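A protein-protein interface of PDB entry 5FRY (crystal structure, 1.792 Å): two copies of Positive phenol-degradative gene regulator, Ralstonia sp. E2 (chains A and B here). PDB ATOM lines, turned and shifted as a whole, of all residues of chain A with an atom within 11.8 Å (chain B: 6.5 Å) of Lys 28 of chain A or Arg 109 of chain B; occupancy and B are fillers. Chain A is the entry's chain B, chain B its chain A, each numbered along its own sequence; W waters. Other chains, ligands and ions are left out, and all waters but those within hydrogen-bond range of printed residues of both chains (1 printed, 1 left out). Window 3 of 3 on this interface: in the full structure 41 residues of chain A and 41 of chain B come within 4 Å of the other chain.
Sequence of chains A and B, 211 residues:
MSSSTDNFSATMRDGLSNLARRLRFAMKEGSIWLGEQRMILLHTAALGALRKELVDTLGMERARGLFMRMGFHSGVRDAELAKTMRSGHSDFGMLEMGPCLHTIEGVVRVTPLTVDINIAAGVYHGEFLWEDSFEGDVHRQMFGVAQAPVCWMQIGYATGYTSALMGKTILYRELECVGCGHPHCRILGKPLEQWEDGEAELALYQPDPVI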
ATOM      1  N   ARG A  24     -13.894 -36.657  15.375  1.00  0.00           N
ATOM      2  CA  ARG A  24     -14.168 -35.333  14.823  1.00  0.00           C
ATOM      3  C   ARG A  24     -14.645 -34.307  15.862  1.00  0.00           C
ATOM      4  O   ARG A  24     -15.463 -34.613  16.725  1.00  0.00           O
ATOM      5  CB  ARG A  24     -15.209 -35.452  13.709  1.00  0.00           C
ATOM      6  CG  ARG A  24     -15.523 -34.143  13.036  1.00  0.00           C
ATOM      7  CD  ARG A  24     -16.416 -34.372  11.845  1.00  0.00           C
ATOM      8  NE  ARG A  24     -17.782 -34.675  12.247  1.00  0.00           N
ATOM      9  CZ  ARG A  24     -18.236 -35.902  12.473  1.00  0.00           C
ATOM     10  NH1 ARG A  24     -17.427 -36.938  12.325  1.00  0.00           N
ATOM     11  NH2 ARG A  24     -19.498 -36.086  12.834  1.00  0.00           N
ATOM     12  N   PHE A  25     -14.145 -33.080  15.751  1.00  0.00           N
ATOM     13  CA  PHE A  25     -14.493 -32.029  16.696  1.00  0.00           C
ATOM     14  C   PHE A  25     -15.361 -30.962  16.045  1.00  0.00           C
ATOM     15  O   PHE A  25     -14.875 -30.147  15.265  1.00  0.00           O
ATOM     16  CB  PHE A  25     -13.225 -31.410  17.284  1.00  0.00           C
ATOM     17  CG  PHE A  25     -12.475 -32.334  18.193  1.00  0.00           C
ATOM     18  CD1 PHE A  25     -11.693 -33.351  17.670  1.00  0.00           C
ATOM     19  CD2 PHE A  25     -12.556 -32.192  19.569  1.00  0.00           C
ATOM     20  CE1 PHE A  25     -11.000 -34.211  18.506  1.00  0.00           C
ATOM     21  CE2 PHE A  25     -11.865 -33.055  20.410  1.00  0.00           C
ATOM     22  CZ  PHE A  25     -11.096 -34.061  19.877  1.00  0.00           C
ATOM     23  N   ALA A  26     -16.649 -30.981  16.377  1.00  0.00           N
ATOM     24  CA  ALA A  26     -17.614 -30.022  15.846  1.00  0.00           C
ATOM     25  C   ALA A  26     -17.945 -28.921  16.862  1.00  0.00           C
ATOM     26  O   ALA A  26     -18.997 -28.954  17.495  1.00  0.00           O
ATOM     27  CB  ALA A  26     -18.883 -30.749  15.414  1.00  0.00           C
ATOM     28  N   MET A  27     -17.054 -27.941  16.996  1.00  0.00           N
ATOM     29  CA  MET A  27     -17.214 -26.874  17.983  1.00  0.00           C
ATOM     30  C   MET A  27     -18.398 -25.955  17.691  1.00  0.00           C
ATOM     31  O   MET A  27     -18.941 -25.346  18.609  1.00  0.00           O
ATOM     32  CB  MET A  27     -15.937 -26.034  18.079  1.00  0.00           C
ATOM     33  CG  MET A  27     -14.742 -26.781  18.649  1.00  0.00           C
ATOM     34  SD  MET A  27     -13.278 -25.739  18.789  1.00  0.00           S
ATOM     35  CE  MET A  27     -13.527 -25.029  20.401  1.00  0.00           C
ATOM     36  N   LYS A  28     -18.784 -25.842  16.419  1.00  0.00           N
ATOM     37  CA  LYS A  28     -19.976 -25.075  16.052  1.00  0.00           C
ATOM     38  C   LYS A  28     -21.189 -25.611  16.795  1.00  0.00           C
ATOM     39  O   LYS A  28     -22.161 -24.895  17.021  1.00  0.00           O
ATOM     40  CB  LYS A  28     -20.254 -25.138  14.548  1.00  0.00           C
ATOM     41  CG  LYS A  28     -19.081 -24.846  13.631  1.00  0.00           C
ATOM     42  CD  LYS A  28     -19.543 -24.919  12.178  1.00  0.00           C
ATOM     43  CE  LYS A  28     -18.453 -24.484  11.213  1.00  0.00           C
ATOM     44  NZ  LYS A  28     -18.942 -24.494   9.803  1.00  0.00           N
ATOM     45  N   GLU A  29     -21.122 -26.889  17.161  1.00  0.00           N
ATOM     46  CA  GLU A  29     -22.220 -27.545  17.852  1.00  0.00           C
ATOM     47  C   GLU A  29     -21.822 -28.108  19.211  1.00  0.00           C
ATOM     48  O   GLU A  29     -22.516 -28.973  19.747  1.00  0.00           O
ATOM     49  CB  GLU A  29     -22.775 -28.660  16.985  1.00  0.00           C
ATOM     50  CG  GLU A  29     -23.258 -28.181  15.644  1.00  0.00           C
ATOM     51  CD  GLU A  29     -23.574 -29.329  14.747  1.00  0.00           C
ATOM     52  OE1 GLU A  29     -22.851 -30.346  14.846  1.00  0.00           O
ATOM     53  OE2 GLU A  29     -24.549 -29.231  13.969  1.00  0.00           O
ATOM     54  N   GLY A  30     -20.710 -27.610  19.752  1.00  0.00           N
ATOM     55  CA  GLY A  30     -20.215 -28.024  21.054  1.00  0.00           C
ATOM     56  C   GLY A  30     -20.144 -29.533  21.167  1.00  0.00           C
ATOM     57  O   GLY A  30     -20.502 -30.108  22.198  1.00  0.00           O
ATOM     58  N   SER A  31     -19.685 -30.165  20.094  1.00  0.00           N
ATOM     59  CA  SER A  31     -19.763 -31.612  19.974  1.00  0.00           C
ATOM     60  C   SER A  31     -18.468 -32.259  19.523  1.00  0.00           C
ATOM     61  O   SER A  31     -17.649 -31.653  18.816  1.00  0.00           O
ATOM     62  CB  SER A  31     -20.886 -31.996  19.007  1.00  0.00           C
ATOM     63  OG  SER A  31     -22.159 -31.876  19.623  1.00  0.00           O
ATOM     64  N   ILE A  32     -18.305 -33.498  19.969  1.00  0.00           N
ATOM     65  CA  ILE A  32     -17.196 -34.372  19.609  1.00  0.00           C
ATOM     66  C   ILE A  32     -17.814 -35.693  19.174  1.00  0.00           C
ATOM     67  O   ILE A  32     -18.696 -36.234  19.860  1.00  0.00           O
ATOM     68  CB  ILE A  32     -16.217 -34.612  20.790  1.00  0.00           C
ATOM     69  CG1 ILE A  32     -15.581 -33.303  21.273  1.00  0.00           C
ATOM     70  CG2 ILE A  32     -15.149 -35.649  20.414  1.00  0.00           C
ATOM     71  CD1 ILE A  32     -14.812 -33.440  22.599  1.00  0.00           C
ATOM     72  N   TRP A  33     -17.358 -36.220  18.040  1.00  0.00           N
ATOM     73  CA  TRP A  33     -17.898 -37.461  17.522  1.00  0.00           C
ATOM     74  C   TRP A  33     -16.804 -38.483  17.282  1.00  0.00           C
ATOM     75  O   TRP A  33     -15.745 -38.160  16.726  1.00  0.00           O
ATOM     76  CB  TRP A  33     -18.655 -37.222  16.218  1.00  0.00           C
ATOM     77  CG  TRP A  33     -19.740 -36.231  16.342  1.00  0.00           C
ATOM     78  CD1 TRP A  33     -19.647 -34.885  16.145  1.00  0.00           C
ATOM     79  CD2 TRP A  33     -21.099 -36.492  16.717  1.00  0.00           C
ATOM     80  NE1 TRP A  33     -20.869 -34.292  16.362  1.00  0.00           N
ATOM     81  CE2 TRP A  33     -21.773 -35.253  16.715  1.00  0.00           C
ATOM     82  CE3 TRP A  33     -21.808 -37.650  17.040  1.00  0.00           C
ATOM     83  CZ2 TRP A  33     -23.115 -35.147  17.018  1.00  0.00           C
ATOM     84  CZ3 TRP A  33     -23.143 -37.540  17.353  1.00  0.00           C
ATOM     85  CH2 TRP A  33     -23.789 -36.295  17.332  1.00  0.00           C
ATOM     86  N   ARG A  38     -21.533 -39.790  19.965  1.00  0.00           N
ATOM     87  CA  ARG A  38     -21.130 -38.518  20.578  1.00  0.00           C
ATOM     88  C   ARG A  38     -20.328 -38.785  21.850  1.00  0.00           C
ATOM     89  O   ARG A  38     -20.687 -39.641  22.648  1.00  0.00           O
ATOM     90  CB  ARG A  38     -22.347 -37.659  20.892  1.00  0.00           C
ATOM     91  CG  ARG A  38     -22.016 -36.458  21.730  1.00  0.00           C
ATOM     92  CD  ARG A  38     -23.069 -35.373  21.667  1.00  0.00           C
ATOM     93  NE  ARG A  38     -22.607 -34.208  22.400  1.00  0.00           N
ATOM     94  CZ  ARG A  38     -23.336 -33.124  22.637  1.00  0.00           C
ATOM     95  NH1 ARG A  38     -24.583 -33.037  22.188  1.00  0.00           N
ATOM     96  NH2 ARG A  38     -22.818 -32.126  23.331  1.00  0.00           N
ATOM     97  N   MET A  39     -19.246 -38.038  22.022  1.00  0.00           N
ATOM     98  CA  MET A  39     -18.292 -38.244  23.104  1.00  0.00           C
ATOM     99  C   MET A  39     -18.146 -36.952  23.887  1.00  0.00           C
ATOM    100  O   MET A  39     -18.455 -35.889  23.363  1.00  0.00           O
ATOM    101  CB  MET A  39     -16.926 -38.649  22.550  1.00  0.00           C
ATOM    102  CG  MET A  39     -16.972 -39.708  21.433  1.00  0.00           C
ATOM    103  SD  MET A  39     -17.367 -41.316  22.051  1.00  0.00           S
ATOM    104  CE  MET A  39     -15.822 -41.784  22.823  1.00  0.00           C
ATOM    105  N   ILE A  40     -17.625 -37.047  25.105  1.00  0.00           N
ATOM    106  CA  ILE A  40     -17.163 -35.857  25.819  1.00  0.00           C
ATOM    107  C   ILE A  40     -15.754 -36.100  26.286  1.00  0.00           C
ATOM    108  O   ILE A  40     -15.320 -37.247  26.383  1.00  0.00           O
ATOM    109  CB  ILE A  40     -18.034 -35.474  27.036  1.00  0.00           C
ATOM    110  CG1 ILE A  40     -18.194 -36.649  28.011  1.00  0.00           C
ATOM    111  CG2 ILE A  40     -19.394 -34.921  26.559  1.00  0.00           C
ATOM    112  CD1 ILE A  40     -18.826 -36.230  29.370  1.00  0.00           C
ATOM    113  N   PRO B  99     -16.879 -21.173  29.550  1.00  0.00           N
ATOM    114  CA  PRO B  99     -17.704 -21.519  28.390  1.00  0.00           C
ATOM    115  C   PRO B  99     -16.903 -22.132  27.220  1.00  0.00           C
ATOM    116  O   PRO B  99     -17.410 -23.064  26.601  1.00  0.00           O
ATOM    117  CB  PRO B  99     -18.330 -20.177  28.001  1.00  0.00           C
ATOM    118  CG  PRO B  99     -18.428 -19.442  29.302  1.00  0.00           C
ATOM    119  CD  PRO B  99     -17.260 -19.868  30.131  1.00  0.00           C
ATOM    120  N   HIS B 102     -15.802 -25.696  28.203  1.00  0.00           N
ATOM    121  CA  HIS B 102     -16.978 -26.558  28.172  1.00  0.00           C
ATOM    122  C   HIS B 102     -17.283 -27.016  26.748  1.00  0.00           C
ATOM    123  O   HIS B 102     -17.700 -28.153  26.526  1.00  0.00           O
ATOM    124  CB  HIS B 102     -18.189 -25.835  28.764  1.00  0.00           C
ATOM    125  CG  HIS B 102     -18.991 -26.675  29.709  1.00  0.00           C
ATOM    126  ND1 HIS B 102     -20.121 -26.206  30.344  1.00  0.00           N
ATOM    127  CD2 HIS B 102     -18.827 -27.952  30.126  1.00  0.00           C
ATOM    128  CE1 HIS B 102     -20.619 -27.159  31.113  1.00  0.00           C
ATOM    129  NE2 HIS B 102     -19.852 -28.229  30.998  1.00  0.00           N
ATOM    130  N   THR B 103     -17.070 -26.121  25.789  1.00  0.00           N
ATOM    131  CA  THR B 103     -17.305 -26.414  24.404  1.00  0.00           C
ATOM    132  C   THR B 103     -16.255 -27.345  23.851  1.00  0.00           C
ATOM    133  O   THR B 103     -16.591 -28.326  23.251  1.00  0.00           O
ATOM    134  CB  THR B 103     -17.410 -25.137  23.567  1.00  0.00           C
ATOM    135  OG1 THR B 103     -18.325 -24.248  24.165  1.00  0.00           O
ATOM    136  CG2 THR B 103     -17.924 -25.427  22.205  1.00  0.00           C
ATOM    137  N   GLY B 106     -16.757 -30.815  24.350  1.00  0.00           N
ATOM    138  CA  GLY B 106     -17.906 -31.402  23.667  1.00  0.00           C
ATOM    139  C   GLY B 106     -19.118 -31.597  24.561  1.00  0.00           C
ATOM    140  O   GLY B 106     -19.958 -32.454  24.320  1.00  0.00           O
ATOM    141  N   VAL B 107     -19.215 -30.796  25.610  1.00  0.00           N
ATOM    142  CA  VAL B 107     -20.313 -30.916  26.560  1.00  0.00           C
ATOM    143  C   VAL B 107     -21.556 -30.154  26.107  1.00  0.00           C
ATOM    144  O   VAL B 107     -22.692 -30.654  26.180  1.00  0.00           O
ATOM    145  CB  VAL B 107     -19.879 -30.392  27.954  1.00  0.00           C
ATOM    146  CG1 VAL B 107     -21.073 -30.156  28.834  1.00  0.00           C
ATOM    147  CG2 VAL B 107     -18.884 -31.385  28.625  1.00  0.00           C
ATOM    148  N   VAL B 108     -21.322 -28.932  25.657  1.00  0.00           N
ATOM    149  CA  VAL B 108     -22.380 -28.020  25.241  1.00  0.00           C
ATOM    150  C   VAL B 108     -21.764 -26.920  24.413  1.00  0.00           C
ATOM    151  O   VAL B 108     -20.564 -26.650  24.496  1.00  0.00           O
ATOM    152  CB  VAL B 108     -23.139 -27.383  26.437  1.00  0.00           C
ATOM    153  CG1 VAL B 108     -24.055 -26.222  25.979  1.00  0.00           C
ATOM    154  CG2 VAL B 108     -23.980 -28.404  27.126  1.00  0.00           C
ATOM    155  N   ARG B 109     -22.609 -26.304  23.603  1.00  0.00           N
ATOM    156  CA  ARG B 109     -22.284 -25.086  22.899  1.00  0.00           C
ATOM    157  C   ARG B 109     -22.785 -23.893  23.709  1.00  0.00           C
ATOM    158  O   ARG B 109     -23.992 -23.686  23.878  1.00  0.00           O
ATOM    159  CB  ARG B 109     -22.912 -25.095  21.513  1.00  0.00           C
ATOM    160  CG  ARG B 109     -22.994 -23.737  20.896  1.00  0.00           C
ATOM    161  CD  ARG B 109     -21.635 -23.268  20.420  1.00  0.00           C
ATOM    162  NE  ARG B 109     -21.741 -22.009  19.686  1.00  0.00           N
ATOM    163  CZ  ARG B 109     -22.509 -21.834  18.618  1.00  0.00           C
ATOM    164  NH1 ARG B 109     -23.252 -22.836  18.157  1.00  0.00           N
ATOM    165  NH2 ARG B 109     -22.538 -20.656  18.010  1.00  0.00           N
ATOM    166  N   VAL B 110     -21.845 -23.121  24.214  1.00  0.00           N
ATOM    167  CA  VAL B 110     -22.164 -22.089  25.190  1.00  0.00           C
ATOM    168  C   VAL B 110     -22.160 -20.724  24.544  1.00  0.00           C
ATOM    169  O   VAL B 110     -21.268 -20.405  23.757  1.00  0.00           O
ATOM    170  CB  VAL B 110     -21.173 -22.112  26.360  1.00  0.00           C
ATOM    171  CG1 VAL B 110     -21.742 -21.335  27.544  1.00  0.00           C
ATOM    172  CG2 VAL B 110     -20.876 -23.530  26.773  1.00  0.00           C
ATOM    173  N   THR B 111     -23.185 -19.930  24.841  1.00  0.00           N
ATOM    174  CA  THR B 111     -23.201 -18.534  24.428  1.00  0.00           C
ATOM    175  C   THR B 111     -23.511 -17.667  25.630  1.00  0.00           C
ATOM    176  O   THR B 111     -24.608 -17.740  26.183  1.00  0.00           O
ATOM    177  CB  THR B 111     -24.231 -18.266  23.309  1.00  0.00           C
ATOM    178  OG1 THR B 111     -23.875 -19.025  22.150  1.00  0.00           O
ATOM    179  CG2 THR B 111     -24.269 -16.779  22.951  1.00  0.00           C
ATOM    180  N   LEU B 129     -26.664 -18.934  27.313  1.00  0.00           N
ATOM    181  CA  LEU B 129     -27.416 -19.813  26.437  1.00  0.00           C
ATOM    182  C   LEU B 129     -26.651 -21.118  26.224  1.00  0.00           C
ATOM    183  O   LEU B 129     -25.442 -21.101  25.958  1.00  0.00           O
ATOM    184  CB  LEU B 129     -27.673 -19.128  25.099  1.00  0.00           C
ATOM    185  CG  LEU B 129     -28.095 -20.021  23.931  1.00  0.00           C
ATOM    186  CD1 LEU B 129     -29.603 -20.245  23.962  1.00  0.00           C
ATOM    187  CD2 LEU B 129     -27.664 -19.426  22.598  1.00  0.00           C
ATOM    188  N   TRP B 130     -27.352 -22.241  26.337  1.00  0.00           N
ATOM    189  CA  TRP B 130     -26.763 -23.549  26.069  1.00  0.00           C
ATOM    190  C   TRP B 130     -27.434 -24.199  24.868  1.00  0.00           C
ATOM    191  O   TRP B 130     -28.624 -24.448  24.909  1.00  0.00           O
ATOM    192  CB  TRP B 130     -26.905 -24.476  27.276  1.00  0.00           C
ATOM    193  CG  TRP B 130     -25.853 -24.300  28.361  1.00  0.00           C
ATOM    194  CD1 TRP B 130     -24.706 -23.575  28.286  1.00  0.00           C
ATOM    195  CD2 TRP B 130     -25.890 -24.868  29.677  1.00  0.00           C
ATOM    196  NE1 TRP B 130     -24.015 -23.654  29.484  1.00  0.00           N
ATOM    197  CE2 TRP B 130     -24.737 -24.423  30.359  1.00  0.00           C
ATOM    198  CE3 TRP B 130     -26.798 -25.684  30.356  1.00  0.00           C
ATOM    199  CZ2 TRP B 130     -24.443 -24.826  31.659  1.00  0.00           C
ATOM    200  CZ3 TRP B 130     -26.517 -26.042  31.675  1.00  0.00           C
ATOM    201  CH2 TRP B 130     -25.337 -25.636  32.296  1.00  0.00           C
ATOM    202  N   GLU B 131     -26.669 -24.492  23.823  1.00  0.00           N
ATOM    203  CA  GLU B 131     -27.210 -25.225  22.685  1.00  0.00           C
ATOM    204  C   GLU B 131     -26.564 -26.597  22.525  1.00  0.00           C
ATOM    205  O   GLU B 131     -25.338 -26.757  22.670  1.00  0.00           O
ATOM    206  CB  GLU B 131     -27.036 -24.402  21.408  1.00  0.00           C
ATOM    207  CG  GLU B 131     -27.774 -23.074  21.447  1.00  0.00           C
ATOM    208  CD  GLU B 131     -27.570 -22.261  20.186  1.00  0.00           C
ATOM    209  OE1 GLU B 131     -28.327 -22.470  19.210  1.00  0.00           O
ATOM    210  OE2 GLU B 131     -26.645 -21.419  20.168  1.00  0.00           O
ATOM    211  N   ASP B 132     -27.407 -27.584  22.229  1.00  0.00           N
ATOM    212  CA  ASP B 132     -26.962 -28.949  22.002  1.00  0.00           C
ATOM    213  C   ASP B 132     -26.293 -29.513  23.247  1.00  0.00           C
ATOM    214  O   ASP B 132     -25.304 -30.234  23.141  1.00  0.00           O
ATOM    215  CB  ASP B 132     -25.997 -29.014  20.821  1.00  0.00           C
ATOM    216  CG  ASP B 132     -26.647 -28.617  19.512  1.00  0.00           C
ATOM    217  OD1 ASP B 132     -27.871 -28.842  19.352  1.00  0.00           O
ATOM    218  OD2 ASP B 132     -25.925 -28.074  18.645  1.00  0.00           O
ATOM    219  N   SER B 133     -26.828 -29.174  24.419  1.00  0.00           N
ATOM    220  CA  SER B 133     -26.291 -29.712  25.655  1.00  0.00           C
ATOM    221  C   SER B 133     -26.355 -31.232  25.550  1.00  0.00           C
ATOM    222  O   SER B 133     -27.376 -31.792  25.158  1.00  0.00           O
ATOM    223  CB  SER B 133     -27.057 -29.199  26.873  1.00  0.00           C
ATOM    224  OG  SER B 133     -28.213 -29.971  27.102  1.00  0.00           O
HETATM  225  O   HOH W   1     -19.726 -33.927  22.333  1.00  0.00           O
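Water W1 lies within hydrogen-bond range of the backbone carbonyl oxygen (O) of Gly 106 of chain B (2.5 Å), the backbone carbonyl oxygen (O) of Met 39 of chain A (2.6 Å), the backbone NH (N) of Ile 32 of chain A (2.8 Å) and the guanidinium group (NE) of Arg 38 of chain A (2.9 Å).
The backbone carbonyl oxygen of Ile 32 of chain A is in hydrogen-bond range of the backbone NH of Met 39 of chain A.
The backbone NH (N) of Val 107 of chain B sits at hydrogen-bond distance from the backbone carbonyl oxygen (O) of His 102 of chain B, 3.2 Å away.
The backbone carbonyl oxygen of Gly 30 of chain A sits at hydrogen-bond distance from the guanidinium group of Arg 38 of chain A (3.3 Å).
O of Pro 99 of chain B lies within hydrogen-bond range of OG1 of Thr 103 of chain B, at 2.9 Å.
The backbone carbonyl oxygen (O) of Glu 29 of chain A sits at hydrogen-bond distance from the side-chain hydroxyl (OG) of Ser 31 of chain A, 2.9 Å away.
The side-chain hydroxyl (OG1) of Thr 103 of chain B sits close to the backbone carbonyl oxygen (O) of Val 108 of chain B (3.3 Å).
Printed residues of chain B within 4 Å of Lys 28 of chain A: Arg 109 (2.6 Å).
Of the printed residues of chain A, Arg 109 of chain B touches Met 27 (3.9 Å), Lys 28 (2.6 Å), Glu 29 (3.9 Å) and Gly 30 (3.8 Å).
Of chain A, only Gly 30 (3.1 Å), Ile 32 (3.7 Å), Arg 38 (3.0 Å), Met 39 (3.9 Å) and Ile 40 (3.4 Å) come within 4 Å of Gly 106 of chain B.
No residue of chain A comes within 4 Å of Thr 111 of chain B.
No residue of chain A comes within 4 Å of Leu 129 of chain B.
No residue of chain A comes within 4 Å of Glu 131 of chain B.
Asp 132 of chain B touches just these residues of chain A: Glu 29 (3.6 Å) and Arg 38 (3.0 Å).
No residue of chain A comes within 4 Å of Ser 133 of chain B.
Of the printed residues of chain B, Gly 30 of chain A touches Thr 103 (3.6 Å), Gly 106 (3.1 Å), Val 107 (3.7 Å), Val 108 (3.7 Å) and Arg 109 (3.8 Å).
Of the printed residues of chain B, Met 39 of chain A touches Gly 106.
Of the printed residues of chain B, Met 27 of chain A touches Thr 103 (3.7 Å) and Arg 109 (3.9 Å).
Ala 26 of chain A touches none of the printed residues of chain B.
The nearest residue of chain A that does not touch Arg 109 of chain B is Arg 38 of chain A (5.8 Å).
The nearest printed residue of chain B that does not touch Ile 40 of chain A is Val 107 of chain B (4.1 Å).
Among the printed residues, pairs that only touch across the chains: Ile 40 of chain A with Gly 106 of chain B (3.4 Å), Glu 29 of chain A with Asp 132 of chain B (3.6 Å), Gly 30 of chain A with Thr 103 of chain B (3.6 Å), Ile 32 of chain A with Gly 106 of chain B (3.7 Å), Gly 30 of chain A with Val 107 of chain B (3.7 Å), Gly 30 of chain A with Val 108 of chain B (3.7 Å), Met 27 of chain A with Thr 103 of chain B (3.7 Å), Gly 30 of chain A with Arg 109 of chain B (3.8 Å), Met 27 of chain A with Arg 109 of chain B (3.9 Å), Met 39 of chain A with Gly 106 of chain B (3.9 Å) and Glu 29 of chain A with Arg 109 of chain B (3.9 Å).
O of Gly 30 of chain A sits close to O of Gly 106 of chain B.
O of Val 107 of chain B is in hydrogen-bond range of NH2 of Arg 38 of chain A (3.2 Å).
O of Asp 132 of chain B sits at hydrogen-bond distance from NH1 of Arg 38 of chain A (3.0 Å).
NH1 of Arg 109 of chain B lies within hydrogen-bond range of O of Lys 28 of chain A, 2.6 Å away.
The guanidinium group (NH2) of Arg 38 of chain A lies within hydrogen-bond range of the backbone carbonyl oxygen (O) of Gly 106 of chain B (3.0 Å).
Printed residues of chain A that touch a printed residue of chain B: Met 27, Lys 28, Glu 29, Gly 30, Ile 32, Arg 38, Met 39 and Ile 40.
Hydrophobic or aromatic side chains of chain A that line the printed part of chain B: Ile 32 and Ile 40.
Along chain A the printed residues that touch a printed residue of chain B span positions 27 to 40.
Among the printed residues, 16 pairs touch across the chains.
No position is printed for both chains.
Of the 16 pairs that touch across the chains among the printed residues, none has its exchanged pair printed and touching as well.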
